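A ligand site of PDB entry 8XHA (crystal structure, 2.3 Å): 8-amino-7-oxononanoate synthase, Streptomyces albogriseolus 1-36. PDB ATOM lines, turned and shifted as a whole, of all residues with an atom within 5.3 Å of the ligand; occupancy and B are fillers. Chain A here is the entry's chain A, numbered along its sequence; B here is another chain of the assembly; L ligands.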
ATOM      1  N   TYR A  53     -13.464   0.490  16.564  1.00  0.00           N
ATOM      2  CA  TYR A  53     -14.908   0.830  16.425  1.00  0.00           C
ATOM      3  C   TYR A  53     -15.194   1.383  15.016  1.00  0.00           C
ATOM      4  O   TYR A  53     -16.315   1.812  14.800  1.00  0.00           O
ATOM      5  CB  TYR A  53     -15.416   1.695  17.584  1.00  0.00           C
ATOM      6  CG  TYR A  53     -14.629   2.911  18.002  1.00  0.00           C
ATOM      7  CD1 TYR A  53     -14.350   3.939  17.120  1.00  0.00           C
ATOM      8  CD2 TYR A  53     -14.239   3.059  19.320  1.00  0.00           C
ATOM      9  CE1 TYR A  53     -13.662   5.062  17.527  1.00  0.00           C
ATOM     10  CE2 TYR A  53     -13.549   4.176  19.743  1.00  0.00           C
ATOM     11  CZ  TYR A  53     -13.260   5.192  18.843  1.00  0.00           C
ATOM     12  OH  TYR A  53     -12.581   6.293  19.255  1.00  0.00           O
ATOM     13  N   TYR A  55     -16.373   0.209  12.391  1.00  0.00           N
ATOM     14  CA  TYR A  55     -17.047  -1.038  11.980  1.00  0.00           C
ATOM     15  C   TYR A  55     -17.073  -1.248  10.456  1.00  0.00           C
ATOM     16  O   TYR A  55     -17.053  -2.396  10.034  1.00  0.00           O
ATOM     17  CB  TYR A  55     -18.433  -1.046  12.616  1.00  0.00           C
ATOM     18  CG  TYR A  55     -18.419  -0.835  14.105  1.00  0.00           C
ATOM     19  CD1 TYR A  55     -17.826  -1.746  14.945  1.00  0.00           C
ATOM     20  CD2 TYR A  55     -19.011   0.283  14.673  1.00  0.00           C
ATOM     21  CE1 TYR A  55     -17.812  -1.570  16.321  1.00  0.00           C
ATOM     22  CE2 TYR A  55     -19.002   0.483  16.047  1.00  0.00           C
ATOM     23  CZ  TYR A  55     -18.401  -0.447  16.860  1.00  0.00           C
ATOM     24  OH  TYR A  55     -18.389  -0.265  18.221  1.00  0.00           O
ATOM     25  N   SER A 112     -19.004  15.697  19.964  1.00  0.00           N
ATOM     26  CA  SER A 112     -18.988  14.336  20.497  1.00  0.00           C
ATOM     27  C   SER A 112     -20.406  13.894  20.847  1.00  0.00           C
ATOM     28  O   SER A 112     -21.285  14.720  21.091  1.00  0.00           O
ATOM     29  CB  SER A 112     -18.124  14.230  21.767  1.00  0.00           C
ATOM     30  OG  SER A 112     -18.739  14.905  22.848  1.00  0.00           O
ATOM     31  N   CYS A 113     -20.603  12.580  20.864  1.00  0.00           N
ATOM     32  CA  CYS A 113     -21.850  12.038  21.367  1.00  0.00           C
ATOM     33  C   CYS A 113     -22.067  12.393  22.836  1.00  0.00           C
ATOM     34  O   CYS A 113     -23.205  12.633  23.252  1.00  0.00           O
ATOM     35  CB  CYS A 113     -21.878  10.535  21.178  1.00  0.00           C
ATOM     36  SG  CYS A 113     -23.506   9.828  21.490  1.00  0.00           S
ATOM     37  N   SER A 114     -20.998  12.454  23.630  1.00  0.00           N
ATOM     38  CA  SER A 114     -21.142  12.852  25.026  1.00  0.00           C
ATOM     39  C   SER A 114     -21.775  14.236  25.134  1.00  0.00           C
ATOM     40  O   SER A 114     -22.734  14.438  25.894  1.00  0.00           O
ATOM     41  CB  SER A 114     -19.783  12.832  25.708  1.00  0.00           C
ATOM     42  OG  SER A 114     -19.245  11.529  25.628  1.00  0.00           O
ATOM     43  N   ALA A 115     -21.275  15.186  24.341  1.00  0.00           N
ATOM     44  CA  ALA A 115     -21.865  16.518  24.301  1.00  0.00           C
ATOM     45  C   ALA A 115     -23.328  16.458  23.886  1.00  0.00           C
ATOM     46  O   ALA A 115     -24.166  17.175  24.433  1.00  0.00           O
ATOM     47  CB  ALA A 115     -21.078  17.422  23.346  1.00  0.00           C
ATOM     48  N   HIS A 144     -25.037   3.764  28.411  1.00  0.00           N
ATOM     49  CA  HIS A 144     -23.657   4.234  28.485  1.00  0.00           C
ATOM     50  C   HIS A 144     -23.530   5.373  29.488  1.00  0.00           C
ATOM     51  O   HIS A 144     -24.474   6.154  29.680  1.00  0.00           O
ATOM     52  CB  HIS A 144     -23.137   4.710  27.123  1.00  0.00           C
ATOM     53  CG  HIS A 144     -21.681   5.043  27.150  1.00  0.00           C
ATOM     54  ND1 HIS A 144     -21.219   6.320  27.380  1.00  0.00           N
ATOM     55  CD2 HIS A 144     -20.586   4.250  27.054  1.00  0.00           C
ATOM     56  CE1 HIS A 144     -19.892   6.302  27.397  1.00  0.00           C
ATOM     57  NE2 HIS A 144     -19.486   5.056  27.211  1.00  0.00           N
ATOM     58  N   CYS A 146     -21.988   8.114  29.470  1.00  0.00           N
ATOM     59  CA  CYS A 146     -22.171   9.501  29.045  1.00  0.00           C
ATOM     60  C   CYS A 146     -23.602   9.962  29.316  1.00  0.00           C
ATOM     61  O   CYS A 146     -23.812  11.122  29.665  1.00  0.00           O
ATOM     62  CB  CYS A 146     -21.785   9.725  27.568  1.00  0.00           C
ATOM     63  SG  CYS A 146     -22.959   9.187  26.287  1.00  0.00           S
ATOM     64  N   ASP A 186     -29.353   2.298  25.165  1.00  0.00           N
ATOM     65  CA  ASP A 186     -28.460   2.206  23.996  1.00  0.00           C
ATOM     66  C   ASP A 186     -29.146   1.285  22.988  1.00  0.00           C
ATOM     67  O   ASP A 186     -29.695   0.264  23.433  1.00  0.00           O
ATOM     68  CB  ASP A 186     -27.077   1.688  24.384  1.00  0.00           C
ATOM     69  CG  ASP A 186     -26.380   2.498  25.454  1.00  0.00           C
ATOM     70  OD1 ASP A 186     -27.046   3.328  26.092  1.00  0.00           O
ATOM     71  OD2 ASP A 186     -25.178   2.280  25.653  1.00  0.00           O
ATOM     72  N   VAL A 188     -27.587  -0.353  20.526  1.00  0.00           N
ATOM     73  CA  VAL A 188     -26.651  -1.517  20.577  1.00  0.00           C
ATOM     74  C   VAL A 188     -25.746  -1.238  21.768  1.00  0.00           C
ATOM     75  O   VAL A 188     -25.131  -0.165  21.793  1.00  0.00           O
ATOM     76  CB  VAL A 188     -25.841  -1.662  19.280  1.00  0.00           C
ATOM     77  CG1 VAL A 188     -24.742  -2.700  19.403  1.00  0.00           C
ATOM     78  CG2 VAL A 188     -26.734  -1.949  18.079  1.00  0.00           C
ATOM     79  N   SER A 190     -22.711  -0.848  24.233  1.00  0.00           N
ATOM     80  CA  SER A 190     -21.256  -0.655  23.985  1.00  0.00           C
ATOM     81  C   SER A 190     -20.473  -1.939  24.256  1.00  0.00           C
ATOM     82  O   SER A 190     -19.470  -2.158  23.560  1.00  0.00           O
ATOM     83  CB  SER A 190     -20.725   0.488  24.801  1.00  0.00           C
ATOM     84  OG  SER A 190     -20.801   0.198  26.188  1.00  0.00           O
ATOM     85  N   ASP A 215     -29.138   5.759  22.170  1.00  0.00           N
ATOM     86  CA  ASP A 215     -27.728   6.062  21.833  1.00  0.00           C
ATOM     87  C   ASP A 215     -27.364   5.103  20.699  1.00  0.00           C
ATOM     88  O   ASP A 215     -27.253   3.910  20.981  1.00  0.00           O
ATOM     89  CB  ASP A 215     -26.816   5.939  23.053  1.00  0.00           C
ATOM     90  CG  ASP A 215     -25.394   6.427  22.832  1.00  0.00           C
ATOM     91  OD1 ASP A 215     -24.914   6.327  21.694  1.00  0.00           O
ATOM     92  OD2 ASP A 215     -24.801   6.917  23.801  1.00  0.00           O
ATOM     93  N   ALA A 217     -24.597   4.922  18.858  1.00  0.00           N
ATOM     94  CA  ALA A 217     -23.148   4.976  18.547  1.00  0.00           C
ATOM     95  C   ALA A 217     -22.663   3.690  17.885  1.00  0.00           C
ATOM     96  O   ALA A 217     -21.813   3.767  16.994  1.00  0.00           O
ATOM     97  CB  ALA A 217     -22.390   5.243  19.818  1.00  0.00           C
ATOM     98  N   HIS A 218     -23.182   2.549  18.332  1.00  0.00           N
ATOM     99  CA  HIS A 218     -22.747   1.257  17.772  1.00  0.00           C
ATOM    100  C   HIS A 218     -23.817   0.731  16.819  1.00  0.00           C
ATOM    101  O   HIS A 218     -23.777  -0.466  16.512  1.00  0.00           O
ATOM    102  CB  HIS A 218     -22.374   0.321  18.931  1.00  0.00           C
ATOM    103  CG  HIS A 218     -21.496   0.975  19.941  1.00  0.00           C
ATOM    104  ND1 HIS A 218     -20.164   1.211  19.705  1.00  0.00           N
ATOM    105  CD2 HIS A 218     -21.755   1.479  21.167  1.00  0.00           C
ATOM    106  CE1 HIS A 218     -19.633   1.808  20.752  1.00  0.00           C
ATOM    107  NE2 HIS A 218     -20.588   1.976  21.659  1.00  0.00           N
ATOM    108  N   SER A 247     -22.449   8.821  17.789  1.00  0.00           N
ATOM    109  CA  SER A 247     -21.101   9.323  17.502  1.00  0.00           C
ATOM    110  C   SER A 247     -20.876   9.130  16.005  1.00  0.00           C
ATOM    111  O   SER A 247     -21.518   8.251  15.429  1.00  0.00           O
ATOM    112  CB  SER A 247     -20.084   8.606  18.328  1.00  0.00           C
ATOM    113  OG  SER A 247     -20.173   7.203  18.133  1.00  0.00           O
ATOM    114  N   ASN A 249     -17.635   9.021  14.744  1.00  0.00           N
ATOM    115  CA  ASN A 249     -16.191   8.681  14.647  1.00  0.00           C
ATOM    116  C   ASN A 249     -16.013   7.160  14.645  1.00  0.00           C
ATOM    117  O   ASN A 249     -14.881   6.706  14.714  1.00  0.00           O
ATOM    118  CB  ASN A 249     -15.398   9.282  15.802  1.00  0.00           C
ATOM    119  CG  ASN A 249     -15.783   8.697  17.146  1.00  0.00           C
ATOM    120  OD1 ASN A 249     -16.954   8.517  17.440  1.00  0.00           O
ATOM    121  ND2 ASN A 249     -14.786   8.412  17.974  1.00  0.00           N
ATOM    122  N   LYS A 250     -17.109   6.424  14.600  1.00  0.00           N
ATOM    123  CA  LYS A 250     -17.037   4.944  14.669  1.00  0.00           C
ATOM    124  C   LYS A 250     -17.317   4.387  13.261  1.00  0.00           C
ATOM    125  O   LYS A 250     -16.423   4.459  12.426  1.00  0.00           O
ATOM    126  CB  LYS A 250     -17.990   4.455  15.759  1.00  0.00           C
ATOM    127  CG  LYS A 250     -17.642   4.929  17.159  1.00  0.00           C
ATOM    128  CD  LYS A 250     -18.625   4.473  18.221  1.00  0.00           C
ATOM    129  CE  LYS A 250     -18.098   4.623  19.629  1.00  0.00           C
ATOM    130  NZ  LYS A 250     -17.758   6.025  19.950  1.00  0.00           N
ATOM    131  N   GLY A 256     -16.713  13.630  15.786  1.00  0.00           N
ATOM    132  CA  GLY A 256     -17.831  14.299  16.470  1.00  0.00           C
ATOM    133  C   GLY A 256     -19.022  13.412  16.716  1.00  0.00           C
ATOM    134  O   GLY A 256     -18.894  12.187  16.581  1.00  0.00           O
ATOM    135  N   GLY A 257     -20.144  14.017  17.098  1.00  0.00           N
ATOM    136  CA  GLY A 257     -21.382  13.269  17.356  1.00  0.00           C
ATOM    137  C   GLY A 257     -22.573  14.025  16.818  1.00  0.00           C
ATOM    138  O   GLY A 257     -22.364  15.040  16.136  1.00  0.00           O
ATOM    139  N   GLU A 361      -9.471  -5.328  23.590  1.00  0.00           N
ATOM    140  CA  GLU A 361      -9.458  -4.460  24.759  1.00  0.00           C
ATOM    141  C   GLU A 361     -10.066  -5.170  25.970  1.00  0.00           C
ATOM    142  O   GLU A 361     -11.042  -5.915  25.828  1.00  0.00           O
ATOM    143  CB  GLU A 361     -10.224  -3.155  24.494  1.00  0.00           C
ATOM    144  CG  GLU A 361     -11.696  -3.289  24.170  1.00  0.00           C
ATOM    145  CD  GLU A 361     -12.288  -1.970  23.668  1.00  0.00           C
ATOM    146  OE1 GLU A 361     -12.199  -0.955  24.381  1.00  0.00           O
ATOM    147  OE2 GLU A 361     -12.802  -1.941  22.529  1.00  0.00           O
ATOM    148  N   ARG A 376     -13.467  -7.234  24.832  1.00  0.00           N
ATOM    149  CA  ARG A 376     -14.485  -6.644  23.959  1.00  0.00           C
ATOM    150  C   ARG A 376     -13.964  -6.669  22.522  1.00  0.00           C
ATOM    151  O   ARG A 376     -13.240  -5.773  22.098  1.00  0.00           O
ATOM    152  CB  ARG A 376     -14.863  -5.232  24.383  1.00  0.00           C
ATOM    153  CG  ARG A 376     -16.161  -4.743  23.732  1.00  0.00           C
ATOM    154  CD  ARG A 376     -16.298  -3.209  23.766  1.00  0.00           C
ATOM    155  NE  ARG A 376     -15.998  -2.671  25.083  1.00  0.00           N
ATOM    156  CZ  ARG A 376     -15.949  -1.374  25.373  1.00  0.00           C
ATOM    157  NH1 ARG A 376     -16.278  -0.459  24.468  1.00  0.00           N
ATOM    158  NH2 ARG A 376     -15.554  -0.994  26.591  1.00  0.00           N
ATOM    159  N   ARG A 378     -14.657  -6.457  18.456  1.00  0.00           N
ATOM    160  CA  ARG A 378     -15.572  -5.728  17.585  1.00  0.00           C
ATOM    161  C   ARG A 378     -15.291  -6.149  16.158  1.00  0.00           C
ATOM    162  O   ARG A 378     -14.138  -6.112  15.720  1.00  0.00           O
ATOM    163  CB  ARG A 378     -15.410  -4.207  17.741  1.00  0.00           C
ATOM    164  CG  ARG A 378     -15.525  -3.718  19.204  1.00  0.00           C
ATOM    165  CD  ARG A 378     -15.625  -2.212  19.260  1.00  0.00           C
ATOM    166  NE  ARG A 378     -14.937  -1.646  20.415  1.00  0.00           N
ATOM    167  CZ  ARG A 378     -15.363  -0.565  21.056  1.00  0.00           C
ATOM    168  NH1 ARG A 378     -16.523  -0.009  20.774  1.00  0.00           N
ATOM    169  NH2 ARG A 378     -14.596  -0.037  22.007  1.00  0.00           N
ATOM    170  N   LEU B  82      -9.923   3.524  19.277  1.00  0.00           N
ATOM    171  CA  LEU B  82     -10.100   2.990  20.623  1.00  0.00           C
ATOM    172  C   LEU B  82     -10.023   4.135  21.621  1.00  0.00           C
ATOM    173  O   LEU B  82      -9.437   5.192  21.340  1.00  0.00           O
ATOM    174  CB  LEU B  82      -9.003   1.971  20.994  1.00  0.00           C
ATOM    175  CG  LEU B  82      -8.874   0.727  20.140  1.00  0.00           C
ATOM    176  CD1 LEU B  82      -7.545   0.035  20.365  1.00  0.00           C
ATOM    177  CD2 LEU B  82     -10.031  -0.210  20.462  1.00  0.00           C
ATOM    178  N   SER B  83     -10.541   3.891  22.821  1.00  0.00           N
ATOM    179  CA  SER B  83     -10.336   4.811  23.932  1.00  0.00           C
ATOM    180  C   SER B  83      -8.851   5.031  24.180  1.00  0.00           C
ATOM    181  O   SER B  83      -8.033   4.119  24.022  1.00  0.00           O
ATOM    182  CB  SER B  83     -11.002   4.277  25.196  1.00  0.00           C
ATOM    183  OG  SER B  83     -10.470   4.943  26.331  1.00  0.00           O
ATOM    184  N   ARG B  84      -8.505   6.264  24.580  1.00  0.00           N
ATOM    185  CA  ARG B  84      -7.116   6.635  24.883  1.00  0.00           C
ATOM    186  C   ARG B  84      -6.548   5.861  26.055  1.00  0.00           C
ATOM    187  O   ARG B  84      -5.336   5.851  26.255  1.00  0.00           O
ATOM    188  CB  ARG B  84      -7.008   8.140  25.163  1.00  0.00           C
ATOM    189  CG  ARG B  84      -7.595   8.643  26.506  1.00  0.00           C
ATOM    190  CD  ARG B  84      -7.232  10.130  26.725  1.00  0.00           C
ATOM    191  NE  ARG B  84      -5.794  10.302  26.943  1.00  0.00           N
ATOM    192  CZ  ARG B  84      -5.096  11.382  26.620  1.00  0.00           C
ATOM    193  NH1 ARG B  84      -5.658  12.400  25.984  1.00  0.00           N
ATOM    194  NH2 ARG B  84      -3.808  11.439  26.930  1.00  0.00           N
ATOM    195  N   ASN B 111     -11.710  16.758  23.522  1.00  0.00           N
ATOM    196  CA  ASN B 111     -12.358  17.367  22.372  1.00  0.00           C
ATOM    197  C   ASN B 111     -12.954  18.741  22.677  1.00  0.00           C
ATOM    198  O   ASN B 111     -13.350  19.448  21.733  1.00  0.00           O
ATOM    199  CB  ASN B 111     -13.438  16.442  21.798  1.00  0.00           C
ATOM    200  CG  ASN B 111     -14.476  16.061  22.821  1.00  0.00           C
ATOM    201  OD1 ASN B 111     -14.973  16.913  23.552  1.00  0.00           O
ATOM    202  ND2 ASN B 111     -14.822  14.765  22.886  1.00  0.00           N
ATOM    203  N   MET B 281     -11.867   9.402  29.796  1.00  0.00           N
ATOM    204  CA  MET B 281     -11.859   7.970  29.512  1.00  0.00           C
ATOM    205  C   MET B 281     -12.687   7.589  28.287  1.00  0.00           C
ATOM    206  O   MET B 281     -12.190   6.848  27.429  1.00  0.00           O
ATOM    207  CB  MET B 281     -12.376   7.174  30.724  1.00  0.00           C
ATOM    208  CG  MET B 281     -12.538   5.675  30.415  1.00  0.00           C
ATOM    209  SD  MET B 281     -13.137   4.692  31.839  1.00  0.00           S
ATOM    210  CE  MET B 281     -11.826   4.952  33.020  1.00  0.00           C
ATOM    211  N   TRP B 282     -13.931   8.050  28.190  1.00  0.00           N
ATOM    212  CA  TRP B 282     -14.806   7.518  27.106  1.00  0.00           C
ATOM    213  C   TRP B 282     -15.306   8.546  26.077  1.00  0.00           C
ATOM    214  O   TRP B 282     -16.240   8.201  25.348  1.00  0.00           O
ATOM    215  CB  TRP B 282     -15.982   6.752  27.723  1.00  0.00           C
ATOM    216  CG  TRP B 282     -16.614   7.336  28.946  1.00  0.00           C
ATOM    217  CD1 TRP B 282     -16.611   6.798  30.201  1.00  0.00           C
ATOM    218  CD2 TRP B 282     -17.388   8.544  29.023  1.00  0.00           C
ATOM    219  NE1 TRP B 282     -17.318   7.593  31.059  1.00  0.00           N
ATOM    220  CE2 TRP B 282     -17.804   8.666  30.367  1.00  0.00           C
ATOM    221  CE3 TRP B 282     -17.759   9.533  28.113  1.00  0.00           C
ATOM    222  CZ2 TRP B 282     -18.572   9.741  30.809  1.00  0.00           C
ATOM    223  CZ3 TRP B 282     -18.522  10.596  28.550  1.00  0.00           C
ATOM    224  CH2 TRP B 282     -18.921  10.699  29.878  1.00  0.00           C
ATOM    225  N   SER B 283     -14.729   9.744  25.998  1.00  0.00           N
ATOM    226  CA  SER B 283     -15.148  10.669  24.921  1.00  0.00           C
ATOM    227  C   SER B 283     -14.012  10.788  23.896  1.00  0.00           C
ATOM    228  O   SER B 283     -12.865  10.903  24.323  1.00  0.00           O
ATOM    229  CB  SER B 283     -15.619  12.011  25.404  1.00  0.00           C
ATOM    230  OG  SER B 283     -16.261  12.719  24.358  1.00  0.00           O
ATOM    231  N   GLN B 284     -14.359  10.826  22.624  1.00  0.00           N
ATOM    232  CA  GLN B 284     -13.352  10.785  21.541  1.00  0.00           C
ATOM    233  C   GLN B 284     -12.230  11.804  21.718  1.00  0.00           C
ATOM    234  O   GLN B 284     -12.503  12.924  22.158  1.00  0.00           O
ATOM    235  CB  GLN B 284     -14.030  10.938  20.182  1.00  0.00           C
ATOM    236  CG  GLN B 284     -14.930  12.161  20.044  1.00  0.00           C
ATOM    237  CD  GLN B 284     -15.644  12.091  18.711  1.00  0.00           C
ATOM    238  OE1 GLN B 284     -15.095  12.442  17.677  1.00  0.00           O
ATOM    239  NE2 GLN B 284     -16.871  11.615  18.741  1.00  0.00           N
ATOM    240  N   ARG B 285     -11.020  11.398  21.375  1.00  0.00           N
ATOM    241  CA  ARG B 285      -9.860  12.295  21.428  1.00  0.00           C
ATOM    242  C   ARG B 285      -9.911  13.240  20.249  1.00  0.00           C
ATOM    243  O   ARG B 285     -10.674  12.980  19.310  1.00  0.00           O
ATOM    244  CB  ARG B 285      -8.584  11.451  21.337  1.00  0.00           C
ATOM    245  CG  ARG B 285      -8.493  10.327  22.358  1.00  0.00           C
ATOM    246  CD  ARG B 285      -7.863   9.082  21.757  1.00  0.00           C
ATOM    247  NE  ARG B 285      -8.515   8.674  20.534  1.00  0.00           N
ATOM    248  CZ  ARG B 285      -9.740   8.156  20.468  1.00  0.00           C
ATOM    249  NH1 ARG B 285     -10.440   8.015  21.578  1.00  0.00           N
ATOM    250  NH2 ARG B 285     -10.252   7.802  19.310  1.00  0.00           N
HETATM  251  N1  LIG L   1     -22.290   6.322  23.451  1.00  0.00           N
HETATM  252  C1  LIG L   1     -21.779   5.081  23.509  1.00  0.00           C
HETATM  253  C2  LIG L   1     -22.751   3.905  23.443  1.00  0.00           C
HETATM  254  C3  LIG L   1     -20.399   4.906  23.623  1.00  0.00           C
HETATM  255  O1  LIG L   1     -19.856   3.615  23.696  1.00  0.00           O
HETATM  256  C4  LIG L   1     -19.588   6.002  23.684  1.00  0.00           C
HETATM  257  C5  LIG L   1     -18.069   5.897  23.802  1.00  0.00           C
HETATM  258  C6  LIG L   1     -20.124   7.263  23.630  1.00  0.00           C
HETATM  259  C7  LIG L   1     -21.490   7.401  23.502  1.00  0.00           C
HETATM  260  C8  LIG L   1     -19.266   8.527  23.687  1.00  0.00           C
HETATM  261  O2  LIG L   1     -18.958   8.860  22.364  1.00  0.00           O
HETATM  262  P1  LIG L   1     -18.103  10.211  22.013  1.00  0.00           P
HETATM  263  O3  LIG L   1     -16.635   9.891  21.871  1.00  0.00           O
HETATM  264  O4  LIG L   1     -18.575  10.764  20.698  1.00  0.00           O
HETATM  265  O5  LIG L   1     -18.273  11.228  23.097  1.00  0.00           O
HETATM  266  N2  LIG L   1     -17.618   4.524  23.904  1.00  0.00           N
HETATM  267  C9  LIG L   1     -16.366   4.420  23.192  1.00  0.00           C
HETATM  268  C10 LIG L   1     -15.247   5.190  23.902  1.00  0.00           C
HETATM  269  C11 LIG L   1     -14.658   5.914  22.699  1.00  0.00           C
HETATM  270  C12 LIG L   1     -13.418   6.762  22.929  1.00  0.00           C
HETATM  271  O6  LIG L   1     -13.064   7.141  24.070  1.00  0.00           O
HETATM  272  O7  LIG L   1     -12.756   7.082  21.902  1.00  0.00           O
HETATM  273  C13 LIG L   1     -16.018   2.942  22.994  1.00  0.00           C
HETATM  274  O8  LIG L   1     -16.615   2.337  22.082  1.00  0.00           O
HETATM  275  O9  LIG L   1     -15.188   2.311  23.707  1.00  0.00           O
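NH1 of Arg 376 is in salt-bridge range of O9 of the ligand, at 3.1 Å.
An oxygen (O5) of the ligand is in hydrogen-bond range of the backbone NH (N) of Ser 114 (3.0 Å).
The side-chain amide nitrogen (NE2) of Gln 284 of chain B lies within hydrogen-bond range of an oxygen (O4) of the ligand (2.7 Å).
NE2 of His 218 lies within hydrogen-bond range of O1 of the ligand (2.7 Å).
The side-chain hydroxyl (OG) of Ser 114 lies within hydrogen-bond range of an oxygen (O5) of the ligand.
O7 of the ligand is in hydrogen-bond range of OH of Tyr 53 (2.8 Å).
The backbone NH (N) of Gln 284 of chain B lies within hydrogen-bond range of an oxygen (O3) of the ligand, at 2.6 Å.
An oxygen (O8) of the ligand is in salt-bridge range of the guanidinium group (NH1) of Arg 378 (2.7 Å).
An oxygen (O7) of the ligand lies within salt-bridge range of the guanidinium group of Arg 285 of chain B.
An oxygen (O4) of the ligand is in hydrogen-bond range of the backbone NH of Cys 113.
An oxygen (O5) of the ligand sits at hydrogen-bond distance from the side-chain hydroxyl of Ser 283 of chain B, 2.8 Å away.
A nitrogen (N1) of the ligand sits at hydrogen-bond distance from the side-chain carboxylate (OD2) of Asp 215.
N of Gly 256 lies within hydrogen-bond range of OE1 of Gln 284 of chain B (2.8 Å).
A ring nitrogen (ND1) of His 218 sits at hydrogen-bond distance from the side-chain hydroxyl (OH) of Tyr 55.
OG of Ser 114 is in hydrogen-bond range of OG of Ser 283 of chain B.
O of Gln 284 of chain B sits at hydrogen-bond distance from ND2 of Asn 111 of chain B (3.0 Å).
N of His 144 is in hydrogen-bond range of OD1 of Asp 186 (3.1 Å).
The side-chain hydroxyl of Ser 283 of chain B sits at hydrogen-bond distance from the side-chain amide nitrogen of Asn 111 of chain B (2.9 Å).
The side-chain carboxylate (OD1) of Asp 215 lies within hydrogen-bond range of the side-chain sulfur (SG) of Cys 113 (3.8 Å).
NH1 of Arg 285 of chain B is in hydrogen-bond range of O of Leu 82 of chain B.
The backbone carbonyl oxygen (O) of Met 281 of chain B lies close to an oxygen (O6) of the ligand (3.5 Å).
CB of Ser 112 touches O5 of the ligand (3.3 Å).
His 144 touches the ligand.
Cys 146 touches the ligand (SG to C7, 3.6 Å).
Asp 186 touches the ligand (OD2 to C2, 3.7 Å).
Ser 190 touches the ligand (CB to O1, 3.4 Å).
CB of Ala 217 touches C1 of the ligand, 3.7 Å away.
CB of Ser 247 touches O4 of the ligand, 3.5 Å away.
Lys 250 touches the ligand (CE to O8, 3.7 Å).
Leu 82 of chain B touches the ligand (O to O7, 3.9 Å).
Ser 83 of chain B touches the ligand.
Trp 282 of chain B touches the ligand.
22 residues have an atom within 4 Å of the ligand: Tyr 53, Ser 112, Cys 113, Ser 114, His 144, Cys 146, Asp 186, Ser 190, Asp 215, Ala 217, His 218, Ser 247, Lys 250, Arg 376, Arg 378, Leu 82 of chain B, Ser 83 of chain B, Met 281 of chain B, Trp 282 of chain B, Ser 283 of chain B, Gln 284 of chain B and Arg 285 of chain B.
The nearest printed residue that does not touch the ligand is Asn 249 (4.3 Å).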
